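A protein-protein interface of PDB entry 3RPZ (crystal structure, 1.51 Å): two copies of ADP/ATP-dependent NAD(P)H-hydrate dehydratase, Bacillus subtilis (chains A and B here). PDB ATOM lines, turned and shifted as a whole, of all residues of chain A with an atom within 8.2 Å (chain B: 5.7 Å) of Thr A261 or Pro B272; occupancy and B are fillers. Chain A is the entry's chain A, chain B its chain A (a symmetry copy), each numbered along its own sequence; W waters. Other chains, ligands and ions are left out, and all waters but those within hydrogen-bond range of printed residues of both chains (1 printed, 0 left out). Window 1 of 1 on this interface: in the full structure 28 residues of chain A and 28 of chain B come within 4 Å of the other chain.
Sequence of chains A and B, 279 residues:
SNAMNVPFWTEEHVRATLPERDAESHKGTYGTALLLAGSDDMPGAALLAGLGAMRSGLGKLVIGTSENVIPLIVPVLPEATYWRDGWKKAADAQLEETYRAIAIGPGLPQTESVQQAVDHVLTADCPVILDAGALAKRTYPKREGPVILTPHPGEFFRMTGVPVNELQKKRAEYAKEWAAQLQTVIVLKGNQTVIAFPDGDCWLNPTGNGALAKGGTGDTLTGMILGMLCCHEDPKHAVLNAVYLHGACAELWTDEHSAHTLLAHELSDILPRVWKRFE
NZ of Lys A214 sits at hydrogen-bond distance from O of Leu A262. ND1 of His A257 sits at hydrogen-bond distance from O of Trp A253 (2.7 Å). The indole nitrogen (NE1) of Trp A253 sits at hydrogen-bond distance from the backbone carbonyl oxygen (O) of Ser A258 (3.1 Å). N of His A260 lies close to OG of Ser A258 (3.1 Å). O of Ser A258 lies within hydrogen-bond range of OG1 of Thr A261 (2.8 Å). The guanidinium group (NE) of Arg B55 sits at hydrogen-bond distance from the backbone carbonyl oxygen (O) of Ser B268, 3.0 Å away.
The side-chain amino group of Lys A214 lies within hydrogen-bond range of the backbone carbonyl oxygen of Met B54. The backbone carbonyl oxygen of Thr A254 lies within hydrogen-bond range of the side-chain amino group of Lys B276 (2.9 Å). The guanidinium group (NH1) of Arg B273 lies within salt-bridge range of the side-chain carboxylate (OE2) of Glu A256. The backbone NH (N) of Ser A258 sits at hydrogen-bond distance from the backbone carbonyl oxygen (O) of Pro B272, 3.0 Å away. N of Gly B57 lies within hydrogen-bond range of O of His A260. The guanidinium group (NH1) of Arg B55 lies within hydrogen-bond range of the backbone carbonyl oxygen (O) of Thr A261 (2.8 Å). The side-chain carboxylate (OE1) of Glu A266 is in salt-bridge range of the guanidinium group (NH1) of Arg B55 (2.8 Å). O of His A260 lies close to O of Arg B55 (3.5 Å).
No position is printed for both chains. Of the 22 pairs that touch across the chains among the printed residues, none has its exchanged pair printed and touching as well.
Printed residues of chain B within 4 Å of Asp A255: Lys B276. Of the printed residues of chain B, Glu A256 touches Arg B273 and Lys B276. Printed residues of chain B within 4 Å of Ser A258: Pro B272, Trp B275 and Lys B276. Thr A261 touches just these residues of chain B: Arg B55 (2.8 Å), Pro B272 (3.2 Å) and Trp B275 (3.5 Å). Printed residues of chain B within 4 Å of Leu A263: Met B54 and Arg B55. Ser B56 touches none of the printed residues of chain A. Printed residues of chain A within 4 Å of Pro B272: Trp A253, His A257, Ser A258 and Thr A261. The nearest residue of chain B that does not touch Thr A261 is Leu B271 (4.5 Å).
Arg B55 touches Trp A253. CZ2 of Trp A253 touches CB of Pro B272, 3.6 Å away. Lys B276 touches Asp A255. CA of His A257 touches O of Pro B272, at 3.4 Å. Arg B273 touches His A257. His A257 touches Lys B276. N of Ser A258 touches CB of Lys B276, 3.7 Å away. CG2 of Thr A261 touches CE3 of Trp B275, 3.5 Å away. Leu A263 touches Met B54. Leu A263 touches Arg B55.
Water W1 bridges O of Glu A256 and O of Arg B273.
Hydrophobic or aromatic side chains of chain B that line the printed part of chain A: Met B54, Pro B272 and Trp B275. Of the 17 printed residues of chain A, 11 touch a printed residue of chain B. Hydrophobic or aromatic side chains of chain A that line the printed part of chain B: Trp A253, His A257, His A260 and Leu A263. Among the printed residues, 22 pairs touch across the chains. Among the printed residues, Asp or Glu carboxylates within 4 Å of a Lys or Arg side-chain nitrogen of the other chain: Glu A256 with Arg B273 (3.0 Å) and Glu A266 with Arg B55 (2.8 Å).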
ATOM      1  N   GLY A 210      19.189 -17.371  25.676  1.00  0.00           N
ATOM      2  CA  GLY A 210      18.477 -17.989  24.574  1.00  0.00           C
ATOM      3  C   GLY A 210      17.050 -17.500  24.374  1.00  0.00           C
ATOM      4  O   GLY A 210      16.418 -17.834  23.371  1.00  0.00           O
ATOM      5  N   ALA A 211      16.523 -16.691  25.275  1.00  0.00           N
ATOM      6  CA  ALA A 211      15.229 -16.033  25.005  1.00  0.00           C
ATOM      7  C   ALA A 211      15.303 -15.201  23.760  1.00  0.00           C
ATOM      8  O   ALA A 211      14.285 -14.977  23.081  1.00  0.00           O
ATOM      9  CB  ALA A 211      14.735 -15.232  26.191  1.00  0.00           C
ATOM     10  N   LEU A 212      16.489 -14.714  23.430  1.00  0.00           N
ATOM     11  CA  LEU A 212      16.710 -13.891  22.232  1.00  0.00           C
ATOM     12  C   LEU A 212      16.776 -14.684  20.939  1.00  0.00           C
ATOM     13  O   LEU A 212      16.774 -14.096  19.856  1.00  0.00           O
ATOM     14  CB  LEU A 212      17.977 -13.023  22.383  1.00  0.00           C
ATOM     15  CG  LEU A 212      17.917 -12.001  23.493  1.00  0.00           C
ATOM     16  CD1 LEU A 212      19.297 -11.392  23.701  1.00  0.00           C
ATOM     17  CD2 LEU A 212      16.879 -10.920  23.194  1.00  0.00           C
ATOM     18  N   LYS A 214      15.086 -16.067  18.662  1.00  0.00           N
ATOM     19  CA  LYS A 214      13.727 -16.113  18.063  1.00  0.00           C
ATOM     20  C   LYS A 214      13.596 -14.940  17.128  1.00  0.00           C
ATOM     21  O   LYS A 214      14.117 -13.858  17.372  1.00  0.00           O
ATOM     22  CB  LYS A 214      12.645 -16.121  19.121  1.00  0.00           C
ATOM     23  CG  LYS A 214      11.257 -16.514  18.595  1.00  0.00           C
ATOM     24  CD  LYS A 214      10.182 -16.491  19.632  1.00  0.00           C
ATOM     25  CE  LYS A 214      10.359 -17.535  20.730  1.00  0.00           C
ATOM     26  NZ  LYS A 214       9.408 -17.322  21.851  1.00  0.00           N
ATOM     27  N   TRP A 253      13.540 -10.661  31.672  1.00  0.00           N
ATOM     28  CA  TRP A 253      12.407 -11.530  31.313  1.00  0.00           C
ATOM     29  C   TRP A 253      12.489 -12.864  31.938  1.00  0.00           C
ATOM     30  O   TRP A 253      11.489 -13.397  32.457  1.00  0.00           O
ATOM     31  CB  TRP A 253      12.399 -11.777  29.796  1.00  0.00           C
ATOM     32  CG  TRP A 253      11.354 -12.779  29.267  1.00  0.00           C
ATOM     33  CD1 TRP A 253      11.557 -14.076  28.869  1.00  0.00           C
ATOM     34  CD2 TRP A 253       9.984 -12.504  29.052  1.00  0.00           C
ATOM     35  NE1 TRP A 253      10.394 -14.631  28.431  1.00  0.00           N
ATOM     36  CE2 TRP A 253       9.415 -13.689  28.499  1.00  0.00           C
ATOM     37  CE3 TRP A 253       9.143 -11.390  29.292  1.00  0.00           C
ATOM     38  CZ2 TRP A 253       8.076 -13.751  28.175  1.00  0.00           C
ATOM     39  CZ3 TRP A 253       7.867 -11.448  28.946  1.00  0.00           C
ATOM     40  CH2 TRP A 253       7.319 -12.629  28.376  1.00  0.00           C
ATOM     41  N   THR A 254      13.657 -13.484  31.871  1.00  0.00           N
ATOM     42  CA  THR A 254      13.793 -14.859  32.327  1.00  0.00           C
ATOM     43  C   THR A 254      13.752 -15.024  33.831  1.00  0.00           C
ATOM     44  O   THR A 254      13.672 -16.139  34.357  1.00  0.00           O
ATOM     45  CB  THR A 254      15.002 -15.608  31.711  1.00  0.00           C
ATOM     46  OG1 THR A 254      16.194 -14.816  31.935  1.00  0.00           O
ATOM     47  CG2 THR A 254      14.815 -15.810  30.259  1.00  0.00           C
ATOM     48  N   ASP A 255      13.713 -13.932  34.574  1.00  0.00           N
ATOM     49  CA  ASP A 255      13.576 -14.067  36.023  1.00  0.00           C
ATOM     50  C   ASP A 255      12.248 -14.723  36.384  1.00  0.00           C
ATOM     51  O   ASP A 255      12.194 -15.524  37.281  1.00  0.00           O
ATOM     52  CB  ASP A 255      13.608 -12.723  36.729  1.00  0.00           C
ATOM     53  CG  ASP A 255      14.986 -12.124  36.824  1.00  0.00           C
ATOM     54  OD1 ASP A 255      15.983 -12.803  36.579  1.00  0.00           O
ATOM     55  OD2 ASP A 255      15.038 -10.939  37.155  1.00  0.00           O
ATOM     56  N   GLU A 256      11.179 -14.347  35.697  1.00  0.00           N
ATOM     57  CA  GLU A 256       9.863 -14.876  36.009  1.00  0.00           C
ATOM     58  C   GLU A 256       9.116 -15.472  34.830  1.00  0.00           C
ATOM     59  O   GLU A 256       7.974 -15.903  35.009  1.00  0.00           O
ATOM     60  CB  GLU A 256       8.999 -13.795  36.608  1.00  0.00           C
ATOM     61  CG  GLU A 256       9.493 -13.304  37.940  1.00  0.00           C
ATOM     62  CD  GLU A 256       8.517 -12.299  38.531  1.00  0.00           C
ATOM     63  OE1 GLU A 256       8.502 -11.126  38.091  1.00  0.00           O
ATOM     64  OE2 GLU A 256       7.724 -12.707  39.388  1.00  0.00           O
ATOM     65  N   HIS A 257       9.779 -15.563  33.692  1.00  0.00           N
ATOM     66  CA  HIS A 257       9.154 -16.102  32.473  1.00  0.00           C
ATOM     67  C   HIS A 257      10.091 -17.110  31.835  1.00  0.00           C
ATOM     68  O   HIS A 257      11.316 -16.958  31.875  1.00  0.00           O
ATOM     69  CB  HIS A 257       8.877 -15.016  31.437  1.00  0.00           C
ATOM     70  CG  HIS A 257       8.146 -13.816  31.958  1.00  0.00           C
ATOM     71  ND1 HIS A 257       8.820 -12.779  32.598  1.00  0.00           N
ATOM     72  CD2 HIS A 257       6.834 -13.502  31.996  1.00  0.00           C
ATOM     73  CE1 HIS A 257       7.938 -11.858  32.960  1.00  0.00           C
ATOM     74  NE2 HIS A 257       6.725 -12.265  32.609  1.00  0.00           N
ATOM     75  N   SER A 258       9.554 -18.129  31.168  1.00  0.00           N
ATOM     76  CA  SER A 258      10.413 -19.082  30.459  1.00  0.00           C
ATOM     77  C   SER A 258      11.108 -18.458  29.266  1.00  0.00           C
ATOM     78  O   SER A 258      10.504 -17.732  28.466  1.00  0.00           O
ATOM     79  CB  SER A 258       9.610 -20.317  29.970  1.00  0.00           C
ATOM     80  OG  SER A 258      10.413 -21.079  29.068  1.00  0.00           O
ATOM     81  N   ALA A 259      12.382 -18.797  29.092  1.00  0.00           N
ATOM     82  CA  ALA A 259      13.155 -18.355  27.974  1.00  0.00           C
ATOM     83  C   ALA A 259      12.616 -18.815  26.620  1.00  0.00           C
ATOM     84  O   ALA A 259      12.967 -18.232  25.615  1.00  0.00           O
ATOM     85  CB  ALA A 259      14.648 -18.822  28.108  1.00  0.00           C
ATOM     86  N   HIS A 260      11.762 -19.806  26.596  1.00  0.00           N
ATOM     87  CA  HIS A 260      11.169 -20.235  25.332  1.00  0.00           C
ATOM     88  C   HIS A 260      10.104 -19.317  24.841  1.00  0.00           C
ATOM     89  O   HIS A 260       9.664 -19.461  23.674  1.00  0.00           O
ATOM     90  CB  HIS A 260      10.569 -21.610  25.513  1.00  0.00           C
ATOM     91  CG  HIS A 260      11.587 -22.671  25.734  1.00  0.00           C
ATOM     92  ND1 HIS A 260      12.457 -23.093  24.752  1.00  0.00           N
ATOM     93  CD2 HIS A 260      11.869 -23.406  26.829  1.00  0.00           C
ATOM     94  CE1 HIS A 260      13.242 -24.032  25.242  1.00  0.00           C
ATOM     95  NE2 HIS A 260      12.882 -24.271  26.497  1.00  0.00           N
ATOM     96  N   THR A 261       9.645 -18.373  25.665  1.00  0.00           N
ATOM     97  CA  THR A 261       8.331 -17.730  25.461  1.00  0.00           C
ATOM     98  C   THR A 261       8.416 -16.232  25.152  1.00  0.00           C
ATOM     99  O   THR A 261       7.368 -15.639  24.908  1.00  0.00           O
ATOM    100  CB  THR A 261       7.406 -17.934  26.641  1.00  0.00           C
ATOM    101  OG1 THR A 261       7.893 -17.191  27.792  1.00  0.00           O
ATOM    102  CG2 THR A 261       7.271 -19.406  27.043  1.00  0.00           C
ATOM    103  N   LEU A 262       9.604 -15.615  25.116  1.00  0.00           N
ATOM    104  CA  LEU A 262       9.738 -14.174  24.837  1.00  0.00           C
ATOM    105  C   LEU A 262       9.332 -13.857  23.413  1.00  0.00           C
ATOM    106  O   LEU A 262       9.688 -14.566  22.502  1.00  0.00           O
ATOM    107  CB  LEU A 262      11.164 -13.736  25.073  1.00  0.00           C
ATOM    108  CG  LEU A 262      11.487 -12.257  24.829  1.00  0.00           C
ATOM    109  CD1 LEU A 262      10.795 -11.316  25.797  1.00  0.00           C
ATOM    110  CD2 LEU A 262      13.016 -12.046  24.887  1.00  0.00           C
ATOM    111  N   LEU A 263       8.633 -12.747  23.225  1.00  0.00           N
ATOM    112  CA  LEU A 263       8.424 -12.178  21.881  1.00  0.00           C
ATOM    113  C   LEU A 263       9.237 -10.897  21.803  1.00  0.00           C
ATOM    114  O   LEU A 263       9.250 -10.102  22.742  1.00  0.00           O
ATOM    115  CB  LEU A 263       6.947 -11.898  21.663  1.00  0.00           C
ATOM    116  CG  LEU A 263       6.041 -13.120  21.756  1.00  0.00           C
ATOM    117  CD1 LEU A 263       4.560 -12.757  21.665  1.00  0.00           C
ATOM    118  CD2 LEU A 263       6.389 -14.099  20.615  1.00  0.00           C
ATOM    119  N   ALA A 264       9.880 -10.649  20.670  1.00  0.00           N
ATOM    120  CA  ALA A 264      10.810  -9.549  20.515  1.00  0.00           C
ATOM    121  C   ALA A 264      10.247  -8.221  20.936  1.00  0.00           C
ATOM    122  O   ALA A 264      10.970  -7.427  21.552  1.00  0.00           O
ATOM    123  CB  ALA A 264      11.308  -9.456  19.072  1.00  0.00           C
ATOM    124  N   GLU A 266       8.424  -7.414  23.254  1.00  0.00           N
ATOM    125  CA  GLU A 266       8.442  -7.262  24.691  1.00  0.00           C
ATOM    126  C   GLU A 266       9.779  -6.741  25.219  1.00  0.00           C
ATOM    127  O   GLU A 266       9.829  -6.116  26.258  1.00  0.00           O
ATOM    128  CB  GLU A 266       8.096  -8.564  25.374  1.00  0.00           C
ATOM    129  CG  GLU A 266       6.660  -8.974  25.044  1.00  0.00           C
ATOM    130  CD  GLU A 266       6.295 -10.349  25.561  1.00  0.00           C
ATOM    131  OE1 GLU A 266       7.026 -11.309  25.300  1.00  0.00           O
ATOM    132  OE2 GLU A 266       5.201 -10.449  26.248  1.00  0.00           O
ATOM    133  N   MET B  54       4.396 -18.897  18.472  1.00  0.00           N
ATOM    134  CA  MET B  54       5.590 -18.110  18.754  1.00  0.00           C
ATOM    135  C   MET B  54       5.896 -18.055  20.227  1.00  0.00           C
ATOM    136  O   MET B  54       7.064 -17.915  20.604  1.00  0.00           O
ATOM    137  CB  MET B  54       5.533 -16.732  18.113  1.00  0.00           C
ATOM    138  CG  MET B  54       5.376 -16.797  16.614  1.00  0.00           C
ATOM    139  SD  MET B  54       6.057 -15.345  15.763  1.00  0.00           S
ATOM    140  CE  MET B  54       7.744 -15.741  15.917  1.00  0.00           C
ATOM    141  N   ARG B  55       4.876 -18.168  21.081  1.00  0.00           N
ATOM    142  CA  ARG B  55       5.099 -18.277  22.517  1.00  0.00           C
ATOM    143  C   ARG B  55       5.715 -19.593  22.925  1.00  0.00           C
ATOM    144  O   ARG B  55       6.198 -19.708  24.053  1.00  0.00           O
ATOM    145  CB  ARG B  55       3.758 -18.134  23.236  1.00  0.00           C
ATOM    146  CG  ARG B  55       3.268 -16.720  23.421  1.00  0.00           C
ATOM    147  CD  ARG B  55       4.084 -15.953  24.431  1.00  0.00           C
ATOM    148  NE  ARG B  55       3.495 -14.704  24.778  1.00  0.00           N
ATOM    149  CZ  ARG B  55       4.144 -13.652  25.241  1.00  0.00           C
ATOM    150  NH1 ARG B  55       5.429 -13.642  25.369  1.00  0.00           N
ATOM    151  NH2 ARG B  55       3.447 -12.574  25.570  1.00  0.00           N
ATOM    152  N   SER B  56       5.677 -20.616  22.080  1.00  0.00           N
ATOM    153  CA  SER B  56       5.995 -21.974  22.453  1.00  0.00           C
ATOM    154  C   SER B  56       7.324 -22.489  21.990  1.00  0.00           C
ATOM    155  O   SER B  56       7.520 -23.682  21.773  1.00  0.00           O
ATOM    156  CB  SER B  56       4.860 -22.908  22.094  1.00  0.00           C
ATOM    157  OG  SER B  56       3.706 -22.560  22.875  1.00  0.00           O
ATOM    158  N   GLY B  57       8.307 -21.602  21.826  1.00  0.00           N
ATOM    159  CA  GLY B  57       9.696 -22.024  21.740  1.00  0.00           C
ATOM    160  C   GLY B  57      10.289 -22.311  20.358  1.00  0.00           C
ATOM    161  O   GLY B  57      11.406 -22.796  20.281  1.00  0.00           O
ATOM    162  N   LEU B 267      -4.444 -17.067  27.054  1.00  0.00           N
ATOM    163  CA  LEU B 267      -3.688 -18.272  27.336  1.00  0.00           C
ATOM    164  C   LEU B 267      -2.222 -18.125  26.933  1.00  0.00           C
ATOM    165  O   LEU B 267      -1.318 -18.494  27.699  1.00  0.00           O
ATOM    166  CB  LEU B 267      -4.285 -19.505  26.630  1.00  0.00           C
ATOM    167  CG  LEU B 267      -5.665 -19.926  27.055  1.00  0.00           C
ATOM    168  CD1 LEU B 267      -6.245 -20.892  26.025  1.00  0.00           C
ATOM    169  CD2 LEU B 267      -5.606 -20.575  28.443  1.00  0.00           C
ATOM    170  N   SER B 268      -1.984 -17.565  25.765  1.00  0.00           N
ATOM    171  CA  SER B 268      -0.647 -17.266  25.270  1.00  0.00           C
ATOM    172  C   SER B 268       0.099 -16.230  26.104  1.00  0.00           C
ATOM    173  O   SER B 268       1.301 -16.247  26.181  1.00  0.00           O
ATOM    174  CB  SER B 268      -0.721 -16.751  23.831  1.00  0.00           C
ATOM    175  OG  SER B 268      -1.293 -17.690  23.024  1.00  0.00           O
ATOM    176  N   ASP B 269      -0.646 -15.292  26.658  1.00  0.00           N
ATOM    177  CA  ASP B 269      -0.108 -14.199  27.472  1.00  0.00           C
ATOM    178  C   ASP B 269       0.319 -14.808  28.852  1.00  0.00           C
ATOM    179  O   ASP B 269       1.219 -14.272  29.524  1.00  0.00           O
ATOM    180  CB  ASP B 269      -1.129 -13.045  27.815  1.00  0.00           C
ATOM    181  CG  ASP B 269      -1.719 -12.144  26.662  1.00  0.00           C
ATOM    182  OD1 ASP B 269      -1.149 -12.007  25.587  1.00  0.00           O
ATOM    183  OD2 ASP B 269      -2.827 -11.492  26.965  1.00  0.00           O
ATOM    184  N   ILE B 270      -0.398 -15.838  29.345  1.00  0.00           N
ATOM    185  CA  ILE B 270      -0.199 -16.492  30.662  1.00  0.00           C
ATOM    186  C   ILE B 270       0.923 -17.519  30.597  1.00  0.00           C
ATOM    187  O   ILE B 270       1.644 -17.763  31.572  1.00  0.00           O
ATOM    188  CB  ILE B 270      -1.545 -17.207  31.096  1.00  0.00           C
ATOM    189  CG1 ILE B 270      -2.586 -16.140  31.415  1.00  0.00           C
ATOM    190  CG2 ILE B 270      -1.409 -18.225  32.258  1.00  0.00           C
ATOM    191  CD1 ILE B 270      -4.045 -16.665  31.422  1.00  0.00           C
ATOM    192  N   LEU B 271       1.110 -18.130  29.432  1.00  0.00           N
ATOM    193  CA  LEU B 271       2.067 -19.227  29.264  1.00  0.00           C
ATOM    194  C   LEU B 271       3.486 -18.887  29.730  1.00  0.00           C
ATOM    195  O   LEU B 271       4.162 -19.727  30.307  1.00  0.00           O
ATOM    196  CB  LEU B 271       2.067 -19.716  27.831  1.00  0.00           C
ATOM    197  CG  LEU B 271       2.980 -20.865  27.476  1.00  0.00           C
ATOM    198  CD1 LEU B 271       2.580 -22.160  28.239  1.00  0.00           C
ATOM    199  CD2 LEU B 271       2.901 -21.126  25.965  1.00  0.00           C
ATOM    200  N   PRO B 272       3.964 -17.661  29.457  1.00  0.00           N
ATOM    201  CA  PRO B 272       5.359 -17.380  29.912  1.00  0.00           C
ATOM    202  C   PRO B 272       5.620 -17.658  31.386  1.00  0.00           C
ATOM    203  O   PRO B 272       6.626 -18.266  31.728  1.00  0.00           O
ATOM    204  CB  PRO B 272       5.533 -15.898  29.547  1.00  0.00           C
ATOM    205  CG  PRO B 272       4.697 -15.724  28.312  1.00  0.00           C
ATOM    206  CD  PRO B 272       3.450 -16.561  28.643  1.00  0.00           C
ATOM    207  N   ARG B 273       4.691 -17.236  32.244  1.00  0.00           N
ATOM    208  CA  ARG B 273       4.839 -17.409  33.679  1.00  0.00           C
ATOM    209  C   ARG B 273       4.532 -18.853  34.090  1.00  0.00           C
ATOM    210  O   ARG B 273       5.197 -19.395  35.002  1.00  0.00           O
ATOM    211  CB  ARG B 273       3.964 -16.417  34.450  1.00  0.00           C
ATOM    212  CG  ARG B 273       4.535 -15.034  34.517  1.00  0.00           C
ATOM    213  CD  ARG B 273       3.660 -14.069  35.393  1.00  0.00           C
ATOM    214  NE  ARG B 273       4.286 -12.745  35.414  1.00  0.00           N
ATOM    215  CZ  ARG B 273       5.218 -12.367  36.271  1.00  0.00           C
ATOM    216  NH1 ARG B 273       5.640 -13.198  37.223  1.00  0.00           N
ATOM    217  NH2 ARG B 273       5.733 -11.143  36.179  1.00  0.00           N
ATOM    218  N   VAL B 274       3.540 -19.450  33.451  1.00  0.00           N
ATOM    219  CA  VAL B 274       3.200 -20.831  33.763  1.00  0.00           C
ATOM    220  C   VAL B 274       4.332 -21.773  33.403  1.00  0.00           C
ATOM    221  O   VAL B 274       4.756 -22.605  34.215  1.00  0.00           O
ATOM    222  CB  VAL B 274       1.900 -21.204  33.114  1.00  0.00           C
ATOM    223  CG1 VAL B 274       1.649 -22.723  33.162  1.00  0.00           C
ATOM    224  CG2 VAL B 274       0.723 -20.447  33.761  1.00  0.00           C
ATOM    225  N   TRP B 275       4.912 -21.626  32.229  1.00  0.00           N
ATOM    226  CA  TRP B 275       5.987 -22.487  31.805  1.00  0.00           C
ATOM    227  C   TRP B 275       7.176 -22.330  32.751  1.00  0.00           C
ATOM    228  O   TRP B 275       7.803 -23.313  33.122  1.00  0.00           O
ATOM    229  CB  TRP B 275       6.355 -22.149  30.335  1.00  0.00           C
ATOM    230  CG  TRP B 275       7.317 -23.038  29.613  1.00  0.00           C
ATOM    231  CD1 TRP B 275       8.351 -23.759  30.099  1.00  0.00           C
ATOM    232  CD2 TRP B 275       7.277 -23.275  28.219  1.00  0.00           C
ATOM    233  NE1 TRP B 275       9.014 -24.431  29.072  1.00  0.00           N
ATOM    234  CE2 TRP B 275       8.347 -24.146  27.907  1.00  0.00           C
ATOM    235  CE3 TRP B 275       6.449 -22.822  27.208  1.00  0.00           C
ATOM    236  CZ2 TRP B 275       8.593 -24.569  26.580  1.00  0.00           C
ATOM    237  CZ3 TRP B 275       6.695 -23.242  25.917  1.00  0.00           C
ATOM    238  CH2 TRP B 275       7.759 -24.096  25.626  1.00  0.00           C
ATOM    239  N   LYS B 276       7.499 -21.127  33.210  1.00  0.00           N
ATOM    240  CA  LYS B 276       8.601 -20.932  34.151  1.00  0.00           C
ATOM    241  C   LYS B 276       8.458 -21.791  35.429  1.00  0.00           C
ATOM    242  O   LYS B 276       9.445 -22.267  35.936  1.00  0.00           O
ATOM    243  CB  LYS B 276       8.680 -19.464  34.520  1.00  0.00           C
ATOM    244  CG  LYS B 276       9.764 -19.041  35.526  1.00  0.00           C
ATOM    245  CD  LYS B 276      11.179 -19.137  34.896  1.00  0.00           C
ATOM    246  CE  LYS B 276      12.288 -18.778  35.897  1.00  0.00           C
ATOM    247  NZ  LYS B 276      13.633 -18.870  35.282  1.00  0.00           N
ATOM    248  N   ARG B 277       7.229 -21.969  35.879  1.00  0.00           N
ATOM    249  CA  ARG B 277       6.924 -22.741  37.093  1.00  0.00           C
ATOM    250  C   ARG B 277       7.375 -24.175  36.990  1.00  0.00           C
ATOM    251  O   ARG B 277       7.622 -24.842  38.019  1.00  0.00           O
ATOM    252  CB  ARG B 277       5.423 -22.751  37.363  1.00  0.00           C
ATOM    253  CG  ARG B 277       5.056 -23.467  38.668  1.00  0.00           C
ATOM    254  CD  ARG B 277       3.686 -23.042  39.136  1.00  0.00           C
ATOM    255  NE  ARG B 277       2.640 -23.950  38.694  1.00  0.00           N
ATOM    256  CZ  ARG B 277       2.499 -25.193  39.140  1.00  0.00           C
ATOM    257  NH1 ARG B 277       3.368 -25.693  40.007  1.00  0.00           N
ATOM    258  NH2 ARG B 277       1.505 -25.948  38.705  1.00  0.00           N
HETATM  259  O   HOH W   1       6.757 -17.565  36.932  1.00  0.00           O
